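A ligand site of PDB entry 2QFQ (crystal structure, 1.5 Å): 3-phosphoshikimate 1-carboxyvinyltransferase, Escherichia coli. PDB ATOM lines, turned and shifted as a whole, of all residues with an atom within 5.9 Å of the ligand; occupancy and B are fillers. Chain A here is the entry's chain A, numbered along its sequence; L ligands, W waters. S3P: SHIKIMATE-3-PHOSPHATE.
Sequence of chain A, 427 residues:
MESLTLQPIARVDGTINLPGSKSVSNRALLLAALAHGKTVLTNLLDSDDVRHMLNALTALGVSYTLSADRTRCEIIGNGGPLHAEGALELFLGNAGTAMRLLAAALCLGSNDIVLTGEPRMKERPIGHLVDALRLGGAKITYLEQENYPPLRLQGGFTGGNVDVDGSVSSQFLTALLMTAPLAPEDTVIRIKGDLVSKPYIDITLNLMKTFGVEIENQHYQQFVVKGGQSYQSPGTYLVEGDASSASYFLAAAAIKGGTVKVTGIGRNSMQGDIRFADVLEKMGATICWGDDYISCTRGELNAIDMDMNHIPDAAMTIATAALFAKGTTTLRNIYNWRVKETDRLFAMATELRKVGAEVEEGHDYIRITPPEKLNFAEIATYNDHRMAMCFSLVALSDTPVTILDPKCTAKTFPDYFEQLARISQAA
Thr 97 touches the ligand. Val 168 touches the ligand (O to O8, 3.99 Å). CD2 of Tyr 200 touches C7 of the ligand, at 3.3 Å. Hydrophobic or aromatic side chains that line the ligand: Tyr 200. Within 4 Å of the ligand: Lys 22, Ser 23, Arg 27, Thr 97, Val 168, Ser 169, Ser 170, Gln 171, Ser 197, Tyr 200, Asp 313, Asn 336 and Lys 340. The nearest printed residue that does not touch the ligand is Pro 312 (4.2 Å).
The side-chain carboxylate (OD1) of Asp 313 lies within hydrogen-bond range of an oxygen (O3) of the ligand (2.7 Å). An oxygen (O7) of the ligand is in hydrogen-bond range of the side-chain amide nitrogen of Asn 336. OG of Ser 23 is in hydrogen-bond range of O5 of the ligand (2.7 Å). OG of Ser 169 is in hydrogen-bond range of O8 of the ligand (2.6 Å). NZ of Lys 22 sits at hydrogen-bond distance from O3 of the ligand, at 3.0 Å. O6 of the ligand lies within hydrogen-bond range of OG of Ser 170 (2.6 Å). The side-chain amino group (NZ) of Lys 340 lies within salt-bridge range of an oxygen (O7) of the ligand (2.8 Å). NH1 of Arg 27 is in salt-bridge range of O4 of the ligand, at 2.7 Å. OG of Ser 197 lies within hydrogen-bond range of O7 of the ligand, at 2.6 Å. NE2 of Gln 171 is in hydrogen-bond range of O1 of the ligand. The backbone NH (N) of Ser 170 lies within hydrogen-bond range of an oxygen (O6) of the ligand.
The guanidinium group (NH1) of Arg 27 lies within hydrogen-bond range of the backbone carbonyl oxygen (O) of Tyr 200 (3.3 Å). The guanidinium group (NE) of Arg 386 is in salt-bridge range of the side-chain carboxylate (OD1) of Asp 313, at 3.9 Å. O of Val 168 is in hydrogen-bond range of ND2 of Asn 336 (3.0 Å). NE of Arg 27 sits at hydrogen-bond distance from OG1 of Thr 204 (2.9 Å). O of Ser 23 sits at hydrogen-bond distance from NH2 of Arg 27, at 3.0 Å. OG of Ser 169 is in hydrogen-bond range of N of Gln 171 (3.0 Å). The side-chain amino group (NZ) of Lys 340 is in salt-bridge range of the side-chain carboxylate (OD2) of Asp 313. NH2 of Arg 100 sits at hydrogen-bond distance from OE1 of Gln 171, at 2.9 Å.
Water W1 lies within hydrogen-bond range of an oxygen (O8) of the ligand, the backbone carbonyl oxygen of Val 168 and the side-chain amide nitrogen of Asn 336. Water W2 lies within hydrogen-bond range of an oxygen (O8) of the ligand (2.7 Å), the guanidinium group (NH2) of Arg 100 (2.9 Å) and the side-chain amide nitrogen (NE2) of Gln 171 (3.0 Å). Water W3 lies within hydrogen-bond range of the side-chain hydroxyl of Thr 174, the side-chain hydroxyl of Ser 170, an oxygen (O4) of the ligand, the guanidinium group of Arg 27 and the backbone NH of Gln 171. Water W4 bridges the side-chain carboxylate of Glu 341 and an oxygen (O3) of the ligand.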
ATOM      1  N   LYS A  22      -7.015  20.589  31.194  1.00  0.00           N
ATOM      2  CA  LYS A  22      -6.488  21.114  29.929  1.00  0.00           C
ATOM      3  C   LYS A  22      -5.757  19.989  29.168  1.00  0.00           C
ATOM      4  O   LYS A  22      -5.927  19.856  27.951  1.00  0.00           O
ATOM      5  CB  LYS A  22      -5.505  22.262  30.230  1.00  0.00           C
ATOM      6  CG  LYS A  22      -4.797  22.784  28.974  1.00  0.00           C
ATOM      7  CD  LYS A  22      -3.288  22.447  28.969  1.00  0.00           C
ATOM      8  CE  LYS A  22      -2.510  23.350  29.927  1.00  0.00           C
ATOM      9  NZ  LYS A  22      -1.123  22.816  30.160  1.00  0.00           N
ATOM     10  N   SER A  23      -4.989  19.181  29.886  1.00  0.00           N
ATOM     11  CA  SER A  23      -4.239  18.090  29.265  1.00  0.00           C
ATOM     12  C   SER A  23      -5.155  17.104  28.573  1.00  0.00           C
ATOM     13  O   SER A  23      -4.897  16.695  27.436  1.00  0.00           O
ATOM     14  CB  SER A  23      -3.413  17.372  30.314  1.00  0.00           C
ATOM     15  OG  SER A  23      -2.389  18.224  30.778  1.00  0.00           O
ATOM     16  N   VAL A  24      -6.209  16.714  29.266  1.00  0.00           N
ATOM     17  CA  VAL A  24      -7.158  15.772  28.687  1.00  0.00           C
ATOM     18  C   VAL A  24      -7.960  16.438  27.585  1.00  0.00           C
ATOM     19  O   VAL A  24      -8.178  15.839  26.496  1.00  0.00           O
ATOM     20  CB  VAL A  24      -8.134  15.233  29.786  1.00  0.00           C
ATOM     21  CG1 VAL A  24      -9.225  14.348  29.157  1.00  0.00           C
ATOM     22  CG2 VAL A  24      -7.337  14.448  30.838  1.00  0.00           C
ATOM     23  N   ARG A  27      -6.037  16.761  24.212  1.00  0.00           N
ATOM     24  CA  ARG A  27      -5.791  15.454  23.589  1.00  0.00           C
ATOM     25  C   ARG A  27      -7.127  14.903  23.036  1.00  0.00           C
ATOM     26  O   ARG A  27      -7.185  14.390  21.915  1.00  0.00           O
ATOM     27  CB  ARG A  27      -5.261  14.458  24.622  1.00  0.00           C
ATOM     28  CG  ARG A  27      -3.787  14.663  24.999  1.00  0.00           C
ATOM     29  CD  ARG A  27      -3.500  13.842  26.234  1.00  0.00           C
ATOM     30  NE  ARG A  27      -2.099  13.773  26.618  1.00  0.00           N
ATOM     31  CZ  ARG A  27      -1.402  14.755  27.187  1.00  0.00           C
ATOM     32  NH1 ARG A  27      -0.124  14.548  27.509  1.00  0.00           N
ATOM     33  NH2 ARG A  27      -1.965  15.932  27.436  1.00  0.00           N
ATOM     34  N   THR A  97       0.519  22.407  24.503  1.00  0.00           N
ATOM     35  CA  THR A  97      -0.085  21.142  24.120  1.00  0.00           C
ATOM     36  C   THR A  97      -0.573  21.202  22.681  1.00  0.00           C
ATOM     37  O   THR A  97      -0.352  20.275  21.910  1.00  0.00           O
ATOM     38  CB  THR A  97      -1.237  20.718  25.069  1.00  0.00           C
ATOM     39  OG1 THR A  97      -2.232  21.747  25.155  1.00  0.00           O
ATOM     40  CG2 THR A  97      -0.692  20.426  26.474  1.00  0.00           C
ATOM     41  N   ARG A 100       2.627  21.336  20.205  1.00  0.00           N
ATOM     42  CA  ARG A 100       3.340  20.088  20.029  1.00  0.00           C
ATOM     43  C   ARG A 100       2.460  19.025  19.388  1.00  0.00           C
ATOM     44  O   ARG A 100       2.898  18.344  18.455  1.00  0.00           O
ATOM     45  CB  ARG A 100       3.897  19.579  21.374  1.00  0.00           C
ATOM     46  CG  ARG A 100       5.242  20.215  21.820  1.00  0.00           C
ATOM     47  CD  ARG A 100       5.097  21.720  22.143  1.00  0.00           C
ATOM     48  NE  ARG A 100       6.348  22.277  22.626  1.00  0.00           N
ATOM     49  CZ  ARG A 100       6.711  22.292  23.904  1.00  0.00           C
ATOM     50  NH1 ARG A 100       7.866  22.841  24.267  1.00  0.00           N
ATOM     51  NH2 ARG A 100       5.921  21.736  24.821  1.00  0.00           N
ATOM     52  N   VAL A 168      13.751  16.873  27.831  1.00  0.00           N
ATOM     53  CA  VAL A 168      13.297  18.254  28.022  1.00  0.00           C
ATOM     54  C   VAL A 168      11.777  18.325  28.130  1.00  0.00           C
ATOM     55  O   VAL A 168      11.236  19.024  28.990  1.00  0.00           O
ATOM     56  CB  VAL A 168      13.809  19.160  26.883  1.00  0.00           C
ATOM     57  CG1 VAL A 168      13.176  20.546  26.994  1.00  0.00           C
ATOM     58  CG2 VAL A 168      15.315  19.263  26.939  1.00  0.00           C
ATOM     59  N   SER A 169      11.066  17.624  27.272  1.00  0.00           N
ATOM     60  CA  SER A 169       9.603  17.629  27.342  1.00  0.00           C
ATOM     61  C   SER A 169       8.996  16.293  26.976  1.00  0.00           C
ATOM     62  O   SER A 169       9.392  15.661  25.994  1.00  0.00           O
ATOM     63  CB  SER A 169       9.002  18.690  26.406  1.00  0.00           C
ATOM     64  OG  SER A 169       7.579  18.704  26.520  1.00  0.00           O
ATOM     65  N   SER A 170       8.023  15.862  27.762  1.00  0.00           N
ATOM     66  CA  SER A 170       7.322  14.631  27.457  1.00  0.00           C
ATOM     67  C   SER A 170       6.354  14.895  26.313  1.00  0.00           C
ATOM     68  O   SER A 170       5.848  13.955  25.680  1.00  0.00           O
ATOM     69  CB  SER A 170       6.506  14.151  28.658  1.00  0.00           C
ATOM     70  OG  SER A 170       5.418  15.032  28.949  1.00  0.00           O
ATOM     71  N   GLN A 171       6.050  16.169  26.045  1.00  0.00           N
ATOM     72  CA  GLN A 171       5.086  16.476  24.999  1.00  0.00           C
ATOM     73  C   GLN A 171       5.527  16.039  23.621  1.00  0.00           C
ATOM     74  O   GLN A 171       4.692  15.786  22.759  1.00  0.00           O
ATOM     75  CB  GLN A 171       4.760  17.968  24.991  1.00  0.00           C
ATOM     76  CG  GLN A 171       3.997  18.413  26.214  1.00  0.00           C
ATOM     77  CD  GLN A 171       3.694  19.891  26.170  1.00  0.00           C
ATOM     78  OE1 GLN A 171       3.401  20.434  25.102  1.00  0.00           O
ATOM     79  NE2 GLN A 171       3.800  20.548  27.323  1.00  0.00           N
ATOM     80  N   THR A 174       4.566  12.425  23.495  1.00  0.00           N
ATOM     81  CA  THR A 174       3.121  12.374  23.440  1.00  0.00           C
ATOM     82  C   THR A 174       2.623  12.633  22.012  1.00  0.00           C
ATOM     83  O   THR A 174       1.773  11.899  21.516  1.00  0.00           O
ATOM     84  CB  THR A 174       2.494  13.418  24.401  1.00  0.00           C
ATOM     85  OG1 THR A 174       2.392  12.824  25.696  1.00  0.00           O
ATOM     86  CG2 THR A 174       1.109  13.874  23.893  1.00  0.00           C
ATOM     87  N   VAL A 196      11.355  12.864  31.064  1.00  0.00           N
ATOM     88  CA  VAL A 196      10.802  13.695  32.123  1.00  0.00           C
ATOM     89  C   VAL A 196       9.278  13.752  32.010  1.00  0.00           C
ATOM     90  O   VAL A 196       8.706  13.344  30.998  1.00  0.00           O
ATOM     91  CB  VAL A 196      11.364  15.145  32.100  1.00  0.00           C
ATOM     92  CG1 VAL A 196      12.867  15.111  32.370  1.00  0.00           C
ATOM     93  CG2 VAL A 196      11.036  15.815  30.764  1.00  0.00           C
ATOM     94  N   SER A 197       8.638  14.203  33.074  1.00  0.00           N
ATOM     95  CA  SER A 197       7.185  14.341  33.112  1.00  0.00           C
ATOM     96  C   SER A 197       6.489  13.077  32.650  1.00  0.00           C
ATOM     97  O   SER A 197       5.478  13.119  31.945  1.00  0.00           O
ATOM     98  CB  SER A 197       6.748  15.515  32.223  1.00  0.00           C
ATOM     99  OG  SER A 197       7.204  16.739  32.796  1.00  0.00           O
ATOM    100  N   TYR A 200       2.574  12.192  32.142  1.00  0.00           N
ATOM    101  CA  TYR A 200       1.780  12.718  31.032  1.00  0.00           C
ATOM    102  C   TYR A 200       1.730  11.757  29.862  1.00  0.00           C
ATOM    103  O   TYR A 200       0.817  11.821  29.045  1.00  0.00           O
ATOM    104  CB  TYR A 200       2.293  14.091  30.568  1.00  0.00           C
ATOM    105  CG  TYR A 200       1.958  15.160  31.567  1.00  0.00           C
ATOM    106  CD1 TYR A 200       2.889  15.552  32.536  1.00  0.00           C
ATOM    107  CD2 TYR A 200       0.710  15.794  31.551  1.00  0.00           C
ATOM    108  CE1 TYR A 200       2.570  16.548  33.463  1.00  0.00           C
ATOM    109  CE2 TYR A 200       0.394  16.803  32.477  1.00  0.00           C
ATOM    110  CZ  TYR A 200       1.336  17.162  33.420  1.00  0.00           C
ATOM    111  OH  TYR A 200       1.070  18.188  34.319  1.00  0.00           O
ATOM    112  N   ILE A 203      -1.213   9.670  30.463  1.00  0.00           N
ATOM    113  CA  ILE A 203      -2.449  10.328  30.093  1.00  0.00           C
ATOM    114  C   ILE A 203      -2.665  10.121  28.596  1.00  0.00           C
ATOM    115  O   ILE A 203      -3.759   9.778  28.150  1.00  0.00           O
ATOM    116  CB  ILE A 203      -2.376  11.847  30.377  1.00  0.00           C
ATOM    117  CG1 ILE A 203      -2.241  12.087  31.884  1.00  0.00           C
ATOM    118  CG2 ILE A 203      -3.626  12.540  29.831  1.00  0.00           C
ATOM    119  CD1 ILE A 203      -2.226  13.581  32.244  1.00  0.00           C
ATOM    120  N   THR A 204      -1.610  10.316  27.809  1.00  0.00           N
ATOM    121  CA  THR A 204      -1.699  10.150  26.351  1.00  0.00           C
ATOM    122  C   THR A 204      -2.157   8.752  25.976  1.00  0.00           C
ATOM    123  O   THR A 204      -3.066   8.590  25.160  1.00  0.00           O
ATOM    124  CB  THR A 204      -0.344  10.458  25.737  1.00  0.00           C
ATOM    125  OG1 THR A 204      -0.069  11.831  26.025  1.00  0.00           O
ATOM    126  CG2 THR A 204      -0.338  10.223  24.225  1.00  0.00           C
ATOM    127  N   PRO A 312       5.579  18.497  37.657  1.00  0.00           N
ATOM    128  CA  PRO A 312       6.161  19.819  37.426  1.00  0.00           C
ATOM    129  C   PRO A 312       5.252  21.042  37.554  1.00  0.00           C
ATOM    130  O   PRO A 312       5.699  22.081  38.061  1.00  0.00           O
ATOM    131  CB  PRO A 312       6.777  19.684  36.028  1.00  0.00           C
ATOM    132  CG  PRO A 312       5.886  18.679  35.350  1.00  0.00           C
ATOM    133  CD  PRO A 312       5.644  17.653  36.448  1.00  0.00           C
ATOM    134  N   ASP A 313       4.001  20.922  37.112  1.00  0.00           N
ATOM    135  CA  ASP A 313       3.067  22.059  37.174  1.00  0.00           C
ATOM    136  C   ASP A 313       2.546  22.247  38.597  1.00  0.00           C
ATOM    137  O   ASP A 313       2.669  23.340  39.167  1.00  0.00           O
ATOM    138  CB  ASP A 313       1.883  21.833  36.234  1.00  0.00           C
ATOM    139  CG  ASP A 313       2.267  21.969  34.768  1.00  0.00           C
ATOM    140  OD1 ASP A 313       1.400  21.708  33.914  1.00  0.00           O
ATOM    141  OD2 ASP A 313       3.421  22.326  34.451  1.00  0.00           O
ATOM    142  N   ASN A 336      12.892  21.742  33.549  1.00  0.00           N
ATOM    143  CA  ASN A 336      12.054  22.259  32.487  1.00  0.00           C
ATOM    144  C   ASN A 336      11.071  23.340  32.852  1.00  0.00           C
ATOM    145  O   ASN A 336      10.382  23.889  31.994  1.00  0.00           O
ATOM    146  CB  ASN A 336      11.436  21.140  31.635  1.00  0.00           C
ATOM    147  CG  ASN A 336      10.308  20.423  32.300  1.00  0.00           C
ATOM    148  OD1 ASN A 336       9.764  20.858  33.325  1.00  0.00           O
ATOM    149  ND2 ASN A 336       9.908  19.300  31.684  1.00  0.00           N
ATOM    150  N   LYS A 340       8.962  26.692  29.927  1.00  0.00           N
ATOM    151  CA  LYS A 340       7.512  26.669  29.839  1.00  0.00           C
ATOM    152  C   LYS A 340       6.880  28.040  29.629  1.00  0.00           C
ATOM    153  O   LYS A 340       7.478  28.857  28.941  1.00  0.00           O
ATOM    154  CB  LYS A 340       6.960  25.929  31.050  1.00  0.00           C
ATOM    155  CG  LYS A 340       7.187  24.421  30.837  1.00  0.00           C
ATOM    156  CD  LYS A 340       6.923  23.605  32.064  1.00  0.00           C
ATOM    157  CE  LYS A 340       7.029  22.131  31.644  1.00  0.00           C
ATOM    158  NZ  LYS A 340       6.880  21.218  32.781  1.00  0.00           N
ATOM    159  N   GLU A 341       5.702  28.306  30.190  1.00  0.00           N
ATOM    160  CA  GLU A 341       5.055  29.592  29.955  1.00  0.00           C
ATOM    161  C   GLU A 341       5.985  30.773  30.147  1.00  0.00           C
ATOM    162  O   GLU A 341       5.826  31.815  29.491  1.00  0.00           O
ATOM    163  CB  GLU A 341       3.799  29.721  30.803  1.00  0.00           C
ATOM    164  CG  GLU A 341       2.616  28.958  30.184  1.00  0.00           C
ATOM    165  CD  GLU A 341       2.533  27.463  30.553  1.00  0.00           C
ATOM    166  OE1 GLU A 341       3.581  26.756  30.766  1.00  0.00           O
ATOM    167  OE2 GLU A 341       1.392  26.976  30.600  1.00  0.00           O
ATOM    168  N   ARG A 344      10.101  29.523  34.796  1.00  0.00           N
ATOM    169  CA  ARG A 344       9.483  29.464  36.110  1.00  0.00           C
ATOM    170  C   ARG A 344      10.433  29.409  37.283  1.00  0.00           C
ATOM    171  O   ARG A 344      10.070  29.817  38.390  1.00  0.00           O
ATOM    172  CB  ARG A 344       8.484  28.300  36.152  1.00  0.00           C
ATOM    173  CG  ARG A 344       7.242  28.599  35.279  1.00  0.00           C
ATOM    174  CD  ARG A 344       6.410  27.346  34.993  1.00  0.00           C
ATOM    175  NE  ARG A 344       5.058  27.745  34.595  1.00  0.00           N
ATOM    176  CZ  ARG A 344       4.103  26.910  34.188  1.00  0.00           C
ATOM    177  NH1 ARG A 344       2.905  27.398  33.878  1.00  0.00           N
ATOM    178  NH2 ARG A 344       4.356  25.593  34.081  1.00  0.00           N
ATOM    179  N   ARG A 386       0.025  30.165  36.104  1.00  0.00           N
ATOM    180  CA  ARG A 386       0.387  29.577  37.366  1.00  0.00           C
ATOM    181  C   ARG A 386       1.099  30.488  38.337  1.00  0.00           C
ATOM    182  O   ARG A 386       1.046  30.285  39.551  1.00  0.00           O
ATOM    183  CB  ARG A 386       1.188  28.285  37.163  1.00  0.00           C
ATOM    184  CG  ARG A 386       0.365  27.237  36.385  1.00  0.00           C
ATOM    185  CD  ARG A 386       0.900  25.798  36.560  1.00  0.00           C
ATOM    186  NE  ARG A 386       0.158  24.967  35.610  1.00  0.00           N
ATOM    187  CZ  ARG A 386      -1.120  24.630  35.730  1.00  0.00           C
ATOM    188  NH1 ARG A 386      -1.682  23.910  34.747  1.00  0.00           N
ATOM    189  NH2 ARG A 386      -1.840  24.926  36.819  1.00  0.00           N
HETATM  190  C1  S3P L   1       1.577  18.557  29.635  1.00  0.00           C
HETATM  191  C2  S3P L   1       2.869  18.089  29.983  1.00  0.00           C
HETATM  192  C3  S3P L   1       3.831  18.941  30.783  1.00  0.00           C
HETATM  193  C4  S3P L   1       3.103  20.100  31.521  1.00  0.00           C
HETATM  194  C5  S3P L   1       2.148  20.825  30.579  1.00  0.00           C
HETATM  195  C6  S3P L   1       1.108  19.835  30.066  1.00  0.00           C
HETATM  196  C7  S3P L   1       0.691  17.665  28.806  1.00  0.00           C
HETATM  197  O1  S3P L   1       4.976  19.407  29.900  1.00  0.00           O
HETATM  198  O2  S3P L   1       4.093  20.961  32.101  1.00  0.00           O
HETATM  199  O3  S3P L   1       1.503  21.897  31.263  1.00  0.00           O
HETATM  200  O4  S3P L   1       1.249  16.799  28.114  1.00  0.00           O
HETATM  201  O5  S3P L   1      -0.515  17.824  28.878  1.00  0.00           O
HETATM  202  P1  S3P L   1       6.504  18.784  29.903  1.00  0.00           P
HETATM  203  O6  S3P L   1       6.407  17.387  29.424  1.00  0.00           O
HETATM  204  O7  S3P L   1       6.973  18.865  31.318  1.00  0.00           O
HETATM  205  O8  S3P L   1       7.289  19.623  28.970  1.00  0.00           O
HETATM  206  O   HOH W   1       9.392  21.191  28.804  1.00  0.00           O
HETATM  207  O   HOH W   2       6.454  21.910  27.707  1.00  0.00           O
HETATM  208  O   HOH W   3       3.143  14.861  27.336  1.00  0.00           O
HETATM  209  O   HOH W   4       3.912  23.946  30.621  1.00  0.00           O
